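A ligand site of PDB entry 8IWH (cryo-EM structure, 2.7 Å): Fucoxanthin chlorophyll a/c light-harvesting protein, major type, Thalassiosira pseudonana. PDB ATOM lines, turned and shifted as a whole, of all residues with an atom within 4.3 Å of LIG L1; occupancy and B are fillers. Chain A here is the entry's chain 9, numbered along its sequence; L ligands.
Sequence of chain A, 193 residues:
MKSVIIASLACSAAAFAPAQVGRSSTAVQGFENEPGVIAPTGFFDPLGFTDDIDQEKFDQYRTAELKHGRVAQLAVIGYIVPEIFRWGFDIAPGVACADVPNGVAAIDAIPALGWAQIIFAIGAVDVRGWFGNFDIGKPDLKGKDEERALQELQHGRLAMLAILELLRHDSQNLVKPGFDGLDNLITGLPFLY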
ATOM      1  N   PHE A  44      -2.883 -14.924   5.188  1.00  0.00           N
ATOM      2  CA  PHE A  44      -2.573 -14.628   6.587  1.00  0.00           C
ATOM      3  C   PHE A  44      -1.206 -15.217   6.914  1.00  0.00           C
ATOM      4  O   PHE A  44      -1.085 -16.350   7.370  1.00  0.00           O
ATOM      5  CB  PHE A  44      -3.651 -15.168   7.514  1.00  0.00           C
ATOM      6  CG  PHE A  44      -3.381 -14.918   8.961  1.00  0.00           C
ATOM      7  CD1 PHE A  44      -3.429 -13.631   9.475  1.00  0.00           C
ATOM      8  CD2 PHE A  44      -3.077 -15.959   9.817  1.00  0.00           C
ATOM      9  CE1 PHE A  44      -3.185 -13.393  10.812  1.00  0.00           C
ATOM     10  CE2 PHE A  44      -2.834 -15.731  11.162  1.00  0.00           C
ATOM     11  CZ  PHE A  44      -2.887 -14.443  11.655  1.00  0.00           C
ATOM     12  N   ASP A  45      -0.154 -14.430   6.666  1.00  0.00           N
ATOM     13  CA  ASP A  45       1.204 -14.748   7.092  1.00  0.00           C
ATOM     14  C   ASP A  45       1.817 -13.512   7.729  1.00  0.00           C
ATOM     15  O   ASP A  45       2.745 -12.914   7.186  1.00  0.00           O
ATOM     16  CB  ASP A  45       2.046 -15.242   5.921  1.00  0.00           C
ATOM     17  CG  ASP A  45       3.336 -15.887   6.370  1.00  0.00           C
ATOM     18  OD1 ASP A  45       3.543 -16.032   7.597  1.00  0.00           O
ATOM     19  OD2 ASP A  45       4.159 -16.259   5.497  1.00  0.00           O
ATOM     20  N   PRO A  46       1.295 -13.092   8.892  1.00  0.00           N
ATOM     21  CA  PRO A  46       1.831 -11.868   9.510  1.00  0.00           C
ATOM     22  C   PRO A  46       3.298 -11.964   9.881  1.00  0.00           C
ATOM     23  O   PRO A  46       4.022 -10.965   9.787  1.00  0.00           O
ATOM     24  CB  PRO A  46       0.938 -11.705  10.759  1.00  0.00           C
ATOM     25  CG  PRO A  46       0.455 -13.072  11.054  1.00  0.00           C
ATOM     26  CD  PRO A  46       0.291 -13.761   9.730  1.00  0.00           C
ATOM     27  N   LEU A  47       3.758 -13.147  10.294  1.00  0.00           N
ATOM     28  CA  LEU A  47       5.161 -13.314  10.643  1.00  0.00           C
ATOM     29  C   LEU A  47       6.048 -13.449   9.416  1.00  0.00           C
ATOM     30  O   LEU A  47       7.209 -13.036   9.452  1.00  0.00           O
ATOM     31  CB  LEU A  47       5.334 -14.537  11.554  1.00  0.00           C
ATOM     32  CG  LEU A  47       5.192 -14.313  13.059  1.00  0.00           C
ATOM     33  CD1 LEU A  47       6.262 -13.354  13.564  1.00  0.00           C
ATOM     34  CD2 LEU A  47       3.803 -13.820  13.427  1.00  0.00           C
ATOM     35  N   PHE A  49       6.429 -16.596   7.557  1.00  0.00           N
ATOM     36  CA  PHE A  49       7.109 -17.889   7.647  1.00  0.00           C
ATOM     37  C   PHE A  49       7.538 -18.394   6.269  1.00  0.00           C
ATOM     38  O   PHE A  49       8.651 -18.921   6.124  1.00  0.00           O
ATOM     39  CB  PHE A  49       6.192 -18.911   8.324  1.00  0.00           C
ATOM     40  CG  PHE A  49       6.336 -18.943   9.816  1.00  0.00           C
ATOM     41  CD1 PHE A  49       6.563 -17.782  10.534  1.00  0.00           C
ATOM     42  CD2 PHE A  49       6.251 -20.137  10.507  1.00  0.00           C
ATOM     43  CE1 PHE A  49       6.693 -17.814  11.909  1.00  0.00           C
ATOM     44  CE2 PHE A  49       6.381 -20.179  11.881  1.00  0.00           C
ATOM     45  CZ  PHE A  49       6.603 -19.007  12.578  1.00  0.00           C
ATOM     46  N   HIS A  68      -2.598 -31.796  12.644  1.00  0.00           N
ATOM     47  CA  HIS A  68      -2.916 -31.166  13.926  1.00  0.00           C
ATOM     48  C   HIS A  68      -4.394 -30.768  13.975  1.00  0.00           C
ATOM     49  O   HIS A  68      -5.063 -30.966  15.000  1.00  0.00           O
ATOM     50  CB  HIS A  68      -2.009 -29.960  14.172  1.00  0.00           C
ATOM     51  CG  HIS A  68      -0.727 -30.278  14.890  1.00  0.00           C
ATOM     52  ND1 HIS A  68       0.375 -30.790  14.250  1.00  0.00           N
ATOM     53  CD2 HIS A  68      -0.359 -30.110  16.186  1.00  0.00           C
ATOM     54  CE1 HIS A  68       1.361 -30.955  15.124  1.00  0.00           C
ATOM     55  NE2 HIS A  68       0.937 -30.543  16.308  1.00  0.00           N
ATOM     56  N   VAL A  71      -6.619 -33.999  14.386  1.00  0.00           N
ATOM     57  CA  VAL A  71      -6.596 -34.547  15.746  1.00  0.00           C
ATOM     58  C   VAL A  71      -7.309 -33.614  16.703  1.00  0.00           C
ATOM     59  O   VAL A  71      -7.964 -34.076  17.651  1.00  0.00           O
ATOM     60  CB  VAL A  71      -5.153 -34.853  16.203  1.00  0.00           C
ATOM     61  CG1 VAL A  71      -4.472 -35.784  15.208  1.00  0.00           C
ATOM     62  CG2 VAL A  71      -4.341 -33.588  16.413  1.00  0.00           C
ATOM     63  N   ALA A  72      -7.233 -32.293  16.486  1.00  0.00           N
ATOM     64  CA  ALA A  72      -8.017 -31.371  17.303  1.00  0.00           C
ATOM     65  C   ALA A  72      -9.516 -31.595  17.108  1.00  0.00           C
ATOM     66  O   ALA A  72     -10.290 -31.550  18.072  1.00  0.00           O
ATOM     67  CB  ALA A  72      -7.643 -29.936  16.980  1.00  0.00           C
ATOM     68  N   ALA A  75     -10.412 -34.716  19.064  1.00  0.00           N
ATOM     69  CA  ALA A  75     -10.292 -34.543  20.500  1.00  0.00           C
ATOM     70  C   ALA A  75     -11.378 -33.652  21.070  1.00  0.00           C
ATOM     71  O   ALA A  75     -11.844 -33.880  22.199  1.00  0.00           O
ATOM     72  CB  ALA A  75      -8.919 -33.967  20.848  1.00  0.00           C
ATOM     73  N   TYR A  79     -13.922 -34.987  24.069  1.00  0.00           N
ATOM     74  CA  TYR A  79     -13.959 -34.402  25.430  1.00  0.00           C
ATOM     75  C   TYR A  79     -15.394 -34.355  25.916  1.00  0.00           C
ATOM     76  O   TYR A  79     -15.643 -34.678  27.094  1.00  0.00           O
ATOM     77  CB  TYR A  79     -13.358 -32.996  25.423  1.00  0.00           C
ATOM     78  CG  TYR A  79     -12.087 -32.829  26.220  1.00  0.00           C
ATOM     79  CD1 TYR A  79     -12.125 -32.515  27.573  1.00  0.00           C
ATOM     80  CD2 TYR A  79     -10.849 -32.956  25.619  1.00  0.00           C
ATOM     81  CE1 TYR A  79     -10.963 -32.338  28.305  1.00  0.00           C
ATOM     82  CE2 TYR A  79      -9.674 -32.787  26.343  1.00  0.00           C
ATOM     83  CZ  TYR A  79      -9.730 -32.472  27.682  1.00  0.00           C
ATOM     84  OH  TYR A  79      -8.584 -32.314  28.398  1.00  0.00           O
ATOM     85  N   ASN A 102     -13.375 -38.258  33.195  1.00  0.00           N
ATOM     86  CA  ASN A 102     -13.334 -37.853  31.793  1.00  0.00           C
ATOM     87  C   ASN A 102     -12.141 -36.955  31.495  1.00  0.00           C
ATOM     88  O   ASN A 102     -11.591 -36.996  30.389  1.00  0.00           O
ATOM     89  CB  ASN A 102     -14.630 -37.155  31.410  1.00  0.00           C
ATOM     90  CG  ASN A 102     -14.629 -36.630  29.992  1.00  0.00           C
ATOM     91  OD1 ASN A 102     -14.030 -37.232  29.096  1.00  0.00           O
ATOM     92  ND2 ASN A 102     -15.296 -35.505  29.774  1.00  0.00           N
ATOM     93  N   GLY A 103     -11.735 -36.130  32.455  1.00  0.00           N
ATOM     94  CA  GLY A 103     -10.720 -35.124  32.211  1.00  0.00           C
ATOM     95  C   GLY A 103      -9.313 -35.640  31.989  1.00  0.00           C
ATOM     96  O   GLY A 103      -9.116 -36.817  31.663  1.00  0.00           O
ATOM     97  N   MET A 160      -8.705 -26.619  16.355  1.00  0.00           N
ATOM     98  CA  MET A 160      -7.318 -26.386  16.814  1.00  0.00           C
ATOM     99  C   MET A 160      -7.367 -25.258  17.848  1.00  0.00           C
ATOM    100  O   MET A 160      -6.490 -25.218  18.728  1.00  0.00           O
ATOM    101  CB  MET A 160      -6.417 -25.973  15.648  1.00  0.00           C
ATOM    102  CG  MET A 160      -5.475 -27.062  15.190  1.00  0.00           C
ATOM    103  SD  MET A 160      -4.306 -26.458  13.949  1.00  0.00           S
ATOM    104  CE  MET A 160      -5.434 -25.698  12.776  1.00  0.00           C
ATOM    105  N   ILE A 163      -9.651 -26.527  21.231  1.00  0.00           N
ATOM    106  CA  ILE A 163      -8.941 -27.532  22.017  1.00  0.00           C
ATOM    107  C   ILE A 163      -8.157 -26.856  23.139  1.00  0.00           C
ATOM    108  O   ILE A 163      -8.059 -27.388  24.259  1.00  0.00           O
ATOM    109  CB  ILE A 163      -8.035 -28.379  21.102  1.00  0.00           C
ATOM    110  CG1 ILE A 163      -7.543 -29.631  21.834  1.00  0.00           C
ATOM    111  CG2 ILE A 163      -6.843 -27.592  20.597  1.00  0.00           C
ATOM    112  CD1 ILE A 163      -8.629 -30.609  22.076  1.00  0.00           C
ATOM    113  N   LEU A 164      -7.594 -25.678  22.873  1.00  0.00           N
ATOM    114  CA  LEU A 164      -6.802 -24.979  23.865  1.00  0.00           C
ATOM    115  C   LEU A 164      -7.648 -24.598  25.064  1.00  0.00           C
ATOM    116  O   LEU A 164      -7.218 -24.766  26.215  1.00  0.00           O
ATOM    117  CB  LEU A 164      -6.151 -23.745  23.254  1.00  0.00           C
ATOM    118  CG  LEU A 164      -4.685 -23.926  22.915  1.00  0.00           C
ATOM    119  CD1 LEU A 164      -4.541 -25.086  21.961  1.00  0.00           C
ATOM    120  CD2 LEU A 164      -4.119 -22.656  22.309  1.00  0.00           C
HETATM  121  C1  LIG L   1      -3.107 -31.567  18.652  1.00  0.00           C
HETATM  122  C2  LIG L   1      -4.402 -31.045  19.188  1.00  0.00           C
HETATM  123  C3  LIG L   1      -1.065 -22.954  15.536  1.00  0.00           C
HETATM  124  C4  LIG L   1      -1.231 -21.630  15.482  1.00  0.00           C
HETATM  125  C5  LIG L   1      -2.168 -20.906  16.408  1.00  0.00           C
HETATM  126  C6  LIG L   1      -0.443 -20.867  14.502  1.00  0.00           C
HETATM  127  C7  LIG L   1      -0.929 -19.929  13.687  1.00  0.00           C
HETATM  128  C8  LIG L   1      -0.066 -19.172  12.692  1.00  0.00           C
HETATM  129  C9  LIG L   1       0.321 -19.846  11.380  1.00  0.00           C
HETATM  130  C10 LIG L   1       1.497 -19.126  10.730  1.00  0.00           C
HETATM  131  C11 LIG L   1       1.419 -17.619  10.808  1.00  0.00           C
HETATM  132  C12 LIG L   1       1.719 -17.277  12.250  1.00  0.00           C
HETATM  133  C13 LIG L   1      -4.862 -29.878  18.733  1.00  0.00           C
HETATM  134  C14 LIG L   1       0.728 -17.948  13.121  1.00  0.00           C
HETATM  135  C15 LIG L   1       1.043 -17.644  14.542  1.00  0.00           C
HETATM  136  C16 LIG L   1       0.786 -21.252  11.709  1.00  0.00           C
HETATM  137  C17 LIG L   1      -0.853 -19.871  10.413  1.00  0.00           C
HETATM  138  C18 LIG L   1      -5.157 -31.799  20.207  1.00  0.00           C
HETATM  139  C19 LIG L   1      -4.892 -33.070  20.495  1.00  0.00           C
HETATM  140  C20 LIG L   1      -5.663 -33.746  21.529  1.00  0.00           C
HETATM  141  C21 LIG L   1      -5.677 -35.086  21.654  1.00  0.00           C
HETATM  142  C22 LIG L   1      -4.868 -35.925  20.718  1.00  0.00           C
HETATM  143  C23 LIG L   1      -6.363 -35.626  22.567  1.00  0.00           C
HETATM  144  C24 LIG L   1      -4.121 -29.125  17.731  1.00  0.00           C
HETATM  145  C25 LIG L   1      -6.982 -36.110  23.449  1.00  0.00           C
HETATM  146  C26 LIG L   1      -7.602 -36.603  24.433  1.00  0.00           C
HETATM  147  C27 LIG L   1      -6.876 -36.652  25.755  1.00  0.00           C
HETATM  148  C28 LIG L   1      -7.542 -37.618  26.721  1.00  0.00           C
HETATM  149  C29 LIG L   1      -9.039 -37.348  26.732  1.00  0.00           C
HETATM  150  C30 LIG L   1      -9.562 -37.800  25.383  1.00  0.00           C
HETATM  151  C31 LIG L   1      -8.855 -37.022  24.304  1.00  0.00           C
HETATM  152  C32 LIG L   1      -9.624 -36.720  23.050  1.00  0.00           C
HETATM  153  C33 LIG L   1      -3.473 -28.023  18.094  1.00  0.00           C
HETATM  154  C34 LIG L   1      -5.434 -37.083  25.508  1.00  0.00           C
HETATM  155  C35 LIG L   1      -6.904 -35.241  26.349  1.00  0.00           C
HETATM  156  C36 LIG L   1      -2.716 -27.241  17.109  1.00  0.00           C
HETATM  157  C37 LIG L   1      -2.701 -25.913  17.209  1.00  0.00           C
HETATM  158  C38 LIG L   1      -3.445 -25.238  18.328  1.00  0.00           C
HETATM  159  C39 LIG L   1      -1.951 -25.084  16.248  1.00  0.00           C
HETATM  160  C40 LIG L   1      -1.803 -23.782  16.489  1.00  0.00           C
HETATM  161  O1  LIG L   1      -0.600 -17.850  12.586  1.00  0.00           O
HETATM  162  O2  LIG L   1       2.418 -17.040   9.959  1.00  0.00           O
HETATM  163  O3  LIG L   1      -9.647 -38.109  27.783  1.00  0.00           O
HETATM  164 MG1  LG2 L   2      -2.005 -22.115   9.417  1.00  0.00          MG
HETATM  165  C1  LG2 L   2      -1.837 -20.629   6.292  1.00  0.00           C
HETATM  166  C2  LG2 L   2       0.699 -24.028   8.660  1.00  0.00           C
HETATM  167  C3  LG2 L   2      -2.172 -23.473  12.565  1.00  0.00           C
HETATM  168  C4  LG2 L   2      -4.812 -20.075  10.163  1.00  0.00           C
HETATM  169  N1  LG2 L   2      -0.798 -22.283   7.734  1.00  0.00           N
HETATM  170  C5  LG2 L   2      -0.872 -21.561   6.535  1.00  0.00           C
HETATM  171  C6  LG2 L   2       0.232 -22.001   5.563  1.00  0.00           C
HETATM  172  C7  LG2 L   2       0.942 -23.144   6.314  1.00  0.00           C
HETATM  173  C8  LG2 L   2       0.255 -23.162   7.672  1.00  0.00           C
HETATM  174  C9  LG2 L   2       0.793 -24.460   5.587  1.00  0.00           C
HETATM  175  C10 LG2 L   2       1.202 -20.872   5.270  1.00  0.00           C
HETATM  176  C11 LG2 L   2       1.515 -20.048   6.507  1.00  0.00           C
HETATM  177  C12 LG2 L   2       2.688 -20.623   7.236  1.00  0.00           C
HETATM  178  O1  LG2 L   2       3.495 -21.475   6.854  1.00  0.00           O
HETATM  179  O2  LG2 L   2       2.832 -20.100   8.487  1.00  0.00           O
HETATM  180  N2  LG2 L   2      -0.919 -23.456  10.438  1.00  0.00           N
HETATM  181  C13 LG2 L   2       0.134 -24.154   9.942  1.00  0.00           C
HETATM  182  C14 LG2 L   2       0.624 -25.122  10.971  1.00  0.00           C
HETATM  183  C15 LG2 L   2      -0.184 -24.972  12.072  1.00  0.00           C
HETATM  184  C16 LG2 L   2      -1.174 -23.912  11.744  1.00  0.00           C
HETATM  185  C17 LG2 L   2       1.748 -26.022  10.728  1.00  0.00           C
HETATM  186  C18 LG2 L   2      -0.179 -25.643  13.343  1.00  0.00           C
HETATM  187  C19 LG2 L   2       0.909 -25.970  14.058  1.00  0.00           C
HETATM  188  N3  LG2 L   2      -3.277 -21.836  11.056  1.00  0.00           N
HETATM  189  C20 LG2 L   2      -3.159 -22.494  12.240  1.00  0.00           C
HETATM  190  C21 LG2 L   2      -4.202 -22.046  13.165  1.00  0.00           C
HETATM  191  C22 LG2 L   2      -4.945 -21.083  12.490  1.00  0.00           C
HETATM  192  C23 LG2 L   2      -4.350 -20.951  11.164  1.00  0.00           C
HETATM  193  C24 LG2 L   2      -4.385 -22.544  14.524  1.00  0.00           C
HETATM  194  C25 LG2 L   2      -6.106 -20.341  12.997  1.00  0.00           C
HETATM  195  C26 LG2 L   2      -5.756 -18.911  13.369  1.00  0.00           C
HETATM  196  N4  LG2 L   2      -3.160 -20.744   8.476  1.00  0.00           N
HETATM  197  C27 LG2 L   2      -4.263 -19.962   8.907  1.00  0.00           C
HETATM  198  C28 LG2 L   2      -4.682 -19.074   7.803  1.00  0.00           C
HETATM  199  C29 LG2 L   2      -3.794 -19.297   6.764  1.00  0.00           C
HETATM  200  C30 LG2 L   2      -2.852 -20.324   7.250  1.00  0.00           C
HETATM  201  C31 LG2 L   2      -5.819 -18.159   7.870  1.00  0.00           C
HETATM  202  C32 LG2 L   2      -3.423 -18.962   5.409  1.00  0.00           C
HETATM  203  O3  LG2 L   2      -3.979 -18.220   4.610  1.00  0.00           O
HETATM  204  C33 LG2 L   2      -2.109 -19.744   5.087  1.00  0.00           C
HETATM  205  C34 LG2 L   2      -2.221 -20.557   3.823  1.00  0.00           C
HETATM  206  O4  LG2 L   2      -3.106 -21.355   3.521  1.00  0.00           O
HETATM  207  O5  LG2 L   2      -1.198 -20.356   2.951  1.00  0.00           O
HETATM  208  C35 LG2 L   2      -1.504 -20.432   1.556  1.00  0.00           C
HETATM  209 MG1  LG3 L   3     -12.400 -41.285  23.693  1.00  0.00          MG
HETATM  210  C1  LG3 L   3     -13.156 -43.163  26.511  1.00  0.00           C
HETATM  211  C2  LG3 L   3      -9.115 -41.284  24.585  1.00  0.00           C
HETATM  212  C3  LG3 L   3     -11.680 -39.565  20.820  1.00  0.00           C
HETATM  213  C4  LG3 L   3     -15.829 -41.334  22.805  1.00  0.00           C
HETATM  214  N1  LG3 L   3     -11.339 -42.089  25.300  1.00  0.00           N
HETATM  215  C5  LG3 L   3     -11.828 -42.855  26.367  1.00  0.00           C
HETATM  216  C6  LG3 L   3     -10.701 -43.253  27.321  1.00  0.00           C
HETATM  217  C7  LG3 L   3      -9.458 -42.537  26.737  1.00  0.00           C
HETATM  218  C8  LG3 L   3      -9.981 -41.928  25.446  1.00  0.00           C
HETATM  219  C9  LG3 L   3      -8.920 -41.493  27.677  1.00  0.00           C
HETATM  220  C10 LG3 L   3     -10.456 -44.754  27.364  1.00  0.00           C
HETATM  221  C11 LG3 L   3     -11.018 -45.524  26.179  1.00  0.00           C
HETATM  222  C12 LG3 L   3     -10.114 -45.441  24.989  1.00  0.00           C
HETATM  223  O1  LG3 L   3      -9.082 -46.085  24.762  1.00  0.00           O
HETATM  224  O2  LG3 L   3     -10.533 -44.529  24.063  1.00  0.00           O
HETATM  225  N2  LG3 L   3     -10.727 -40.537  22.879  1.00  0.00           N
HETATM  226  C13 LG3 L   3      -9.471 -40.674  23.373  1.00  0.00           C
HETATM  227  C14 LG3 L   3      -8.483 -40.077  22.432  1.00  0.00           C
HETATM  228  C15 LG3 L   3      -9.207 -39.589  21.362  1.00  0.00           C
HETATM  229  C16 LG3 L   3     -10.635 -39.873  21.630  1.00  0.00           C
HETATM  230  C17 LG3 L   3      -7.048 -40.065  22.703  1.00  0.00           C
HETATM  231  C18 LG3 L   3      -8.779 -38.914  20.168  1.00  0.00           C
HETATM  232  C19 LG3 L   3      -7.765 -38.043  20.075  1.00  0.00           C
HETATM  233  N3  LG3 L   3     -13.559 -40.559  22.118  1.00  0.00           N
HETATM  234  C20 LG3 L   3     -13.046 -39.882  21.047  1.00  0.00           C
HETATM  235  C21 LG3 L   3     -14.130 -39.526  20.130  1.00  0.00           C
HETATM  236  C22 LG3 L   3     -15.301 -40.026  20.691  1.00  0.00           C
HETATM  237  C23 LG3 L   3     -14.931 -40.688  21.941  1.00  0.00           C
HETATM  238  C24 LG3 L   3     -13.959 -38.778  18.886  1.00  0.00           C
HETATM  239  C25 LG3 L   3     -16.651 -39.925  20.120  1.00  0.00           C
HETATM  240  C26 LG3 L   3     -16.999 -41.074  19.212  1.00  0.00           C
HETATM  241  N4  LG3 L   3     -14.131 -42.030  24.443  1.00  0.00           N
HETATM  242  C27 LG3 L   3     -15.474 -41.970  23.983  1.00  0.00           C
HETATM  243  C28 LG3 L   3     -16.342 -42.685  24.950  1.00  0.00           C
HETATM  244  C29 LG3 L   3     -15.507 -43.160  25.933  1.00  0.00           C
HETATM  245  C30 LG3 L   3     -14.144 -42.730  25.572  1.00  0.00           C
HETATM  246  C31 LG3 L   3     -17.785 -42.831  24.817  1.00  0.00           C
HETATM  247  C32 LG3 L   3     -15.410 -43.905  27.175  1.00  0.00           C
HETATM  248  O3  LG3 L   3     -16.290 -44.459  27.816  1.00  0.00           O
HETATM  249  C33 LG3 L   3     -13.902 -43.922  27.583  1.00  0.00           C
HETATM  250  C34 LG3 L   3     -13.683 -43.324  28.941  1.00  0.00           C
HETATM  251  O4  LG3 L   3     -13.790 -42.144  29.277  1.00  0.00           O
HETATM  252  O5  LG3 L   3     -13.310 -44.230  29.889  1.00  0.00           O
HETATM  253  C35 LG3 L   3     -13.763 -43.984  31.224  1.00  0.00           C
HETATM  254  C36 LG3 L   3     -11.716 -44.836  23.302  1.00  0.00           C
HETATM  255  C37 LG3 L   3     -11.290 -44.965  21.890  1.00  0.00           C
HETATM  256  C38 LG3 L   3     -11.950 -44.417  20.852  1.00  0.00           C
HETATM  257  C39 LG3 L   3     -13.181 -43.627  21.029  1.00  0.00           C
HETATM  258  C40 LG3 L   3     -11.466 -44.586  19.459  1.00  0.00           C
HETATM  259  C41 LG3 L   3     -11.673 -43.349  18.604  1.00  0.00           C
HETATM  260  C42 LG3 L   3     -10.797 -43.404  17.373  1.00  0.00           C
HETATM  261  C43 LG3 L   3     -11.454 -42.739  16.172  1.00  0.00           C
HETATM  262  C44 LG3 L   3     -12.871 -43.244  16.008  1.00  0.00           C
HETATM  263  C45 LG3 L   3     -10.656 -43.015  14.901  1.00  0.00           C
HETATM  264 MG1  LG4 L   4       2.432 -30.452  17.487  1.00  0.00          MG
HETATM  265  C1  LG4 L   4       4.958 -30.663  15.106  1.00  0.00           C
HETATM  266  C2  LG4 L   4       2.639 -27.072  17.360  1.00  0.00           C
HETATM  267  C3  LG4 L   4       0.348 -30.300  20.187  1.00  0.00           C
HETATM  268  C4  LG4 L   4       2.470 -33.975  17.768  1.00  0.00           C
HETATM  269  N1  LG4 L   4       3.517 -29.114  16.304  1.00  0.00           N
HETATM  270  C5  LG4 L   4       4.534 -29.392  15.381  1.00  0.00           C
HETATM  271  C6  LG4 L   4       5.050 -28.083  14.767  1.00  0.00           C
HETATM  272  C7  LG4 L   4       4.014 -27.039  15.231  1.00  0.00           C
HETATM  273  C8  LG4 L   4       3.331 -27.762  16.382  1.00  0.00           C
HETATM  274  C9  LG4 L   4       4.658 -25.754  15.684  1.00  0.00           C
HETATM  275  C10 LG4 L   4       5.068 -28.111  13.244  1.00  0.00           C
HETATM  276  C11 LG4 L   4       6.448 -27.746  12.726  1.00  0.00           C
HETATM  277  C12 LG4 L   4       6.884 -28.744  11.690  1.00  0.00           C
HETATM  278  O1  LG4 L   4       7.996 -28.897  11.192  1.00  0.00           O
HETATM  279  O2  LG4 L   4       5.867 -29.570  11.293  1.00  0.00           O
HETATM  280  N2  LG4 L   4       1.496 -28.958  18.453  1.00  0.00           N
HETATM  281  C13 LG4 L   4       1.998 -27.697  18.449  1.00  0.00           C
HETATM  282  C14 LG4 L   4       1.843 -27.044  19.780  1.00  0.00           C
HETATM  283  C15 LG4 L   4       1.194 -27.953  20.570  1.00  0.00           C
HETATM  284  C16 LG4 L   4       0.933 -29.164  19.736  1.00  0.00           C
HETATM  285  C17 LG4 L   4       2.295 -25.693  20.074  1.00  0.00           C
HETATM  286  C18 LG4 L   4       0.776 -27.850  21.950  1.00  0.00           C
HETATM  287  N3  LG4 L   4       1.448 -31.883  18.642  1.00  0.00           N
HETATM  288  C19 LG4 L   4       0.568 -31.596  19.638  1.00  0.00           C
HETATM  289  C20 LG4 L   4       0.003 -32.820  20.188  1.00  0.00           C
HETATM  290  C21 LG4 L   4       0.708 -33.868  19.598  1.00  0.00           C
HETATM  291  C22 LG4 L   4       1.603 -33.271  18.615  1.00  0.00           C
HETATM  292  C23 LG4 L   4      -1.007 -32.877  21.253  1.00  0.00           C
HETATM  293  C24 LG4 L   4       0.511 -35.305  19.816  1.00  0.00           C
HETATM  294  C25 LG4 L   4       1.381 -35.840  20.924  1.00  0.00           C
HETATM  295  N4  LG4 L   4       3.354 -32.013  16.584  1.00  0.00           N
HETATM  296  C26 LG4 L   4       3.304 -33.406  16.829  1.00  0.00           C
HETATM  297  C27 LG4 L   4       4.274 -34.091  15.935  1.00  0.00           C
HETATM  298  C28 LG4 L   4       4.944 -33.081  15.264  1.00  0.00           C
HETATM  299  C29 LG4 L   4       4.346 -31.805  15.716  1.00  0.00           C
HETATM  300  C30 LG4 L   4       4.458 -35.535  15.878  1.00  0.00           C
HETATM  301  C31 LG4 L   4       5.940 -32.761  14.274  1.00  0.00           C
HETATM  302  O3  LG4 L   4       6.611 -33.518  13.573  1.00  0.00           O
HETATM  303  C32 LG4 L   4       6.055 -31.212  14.224  1.00  0.00           C
HETATM  304  C33 LG4 L   4       7.395 -30.744  14.728  1.00  0.00           C
HETATM  305  O4  LG4 L   4       7.719 -30.567  15.901  1.00  0.00           O
HETATM  306  O5  LG4 L   4       8.315 -30.510  13.764  1.00  0.00           O
HETATM  307  C34 LG4 L   4       9.428 -29.684  14.100  1.00  0.00           C
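The side-chain carboxylate (OD1) of Asp 45 sits at hydrogen-bond distance from an oxygen (O2) of LIG L1, 2.8 Å away.
O of Asn 102 lies within hydrogen-bond range of O3 of LIG L1, 3.4 Å away.
NE2 of His 68 binds MG1 of LG4 L4, at 1.9 Å.
An oxygen (O2) of LG2 L2 sits close to an oxygen (O2) of LIG L1 (3.4 Å).
The side-chain carboxylate of Asp 45 lies within hydrogen-bond range of the backbone NH of Phe 49.
The side-chain amide nitrogen of Asn 102 is in hydrogen-bond range of the backbone carbonyl oxygen of Tyr 79 (2.8 Å).
Residues that only touch LIG L1: Phe 44, Pro 46, His 68, Val 71, Ala 72, Ala 75, Tyr 79, Met 160, Ile 163 and Leu 164.
Of the 15 residues printed, 12 come within 4 Å of LIG L1.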
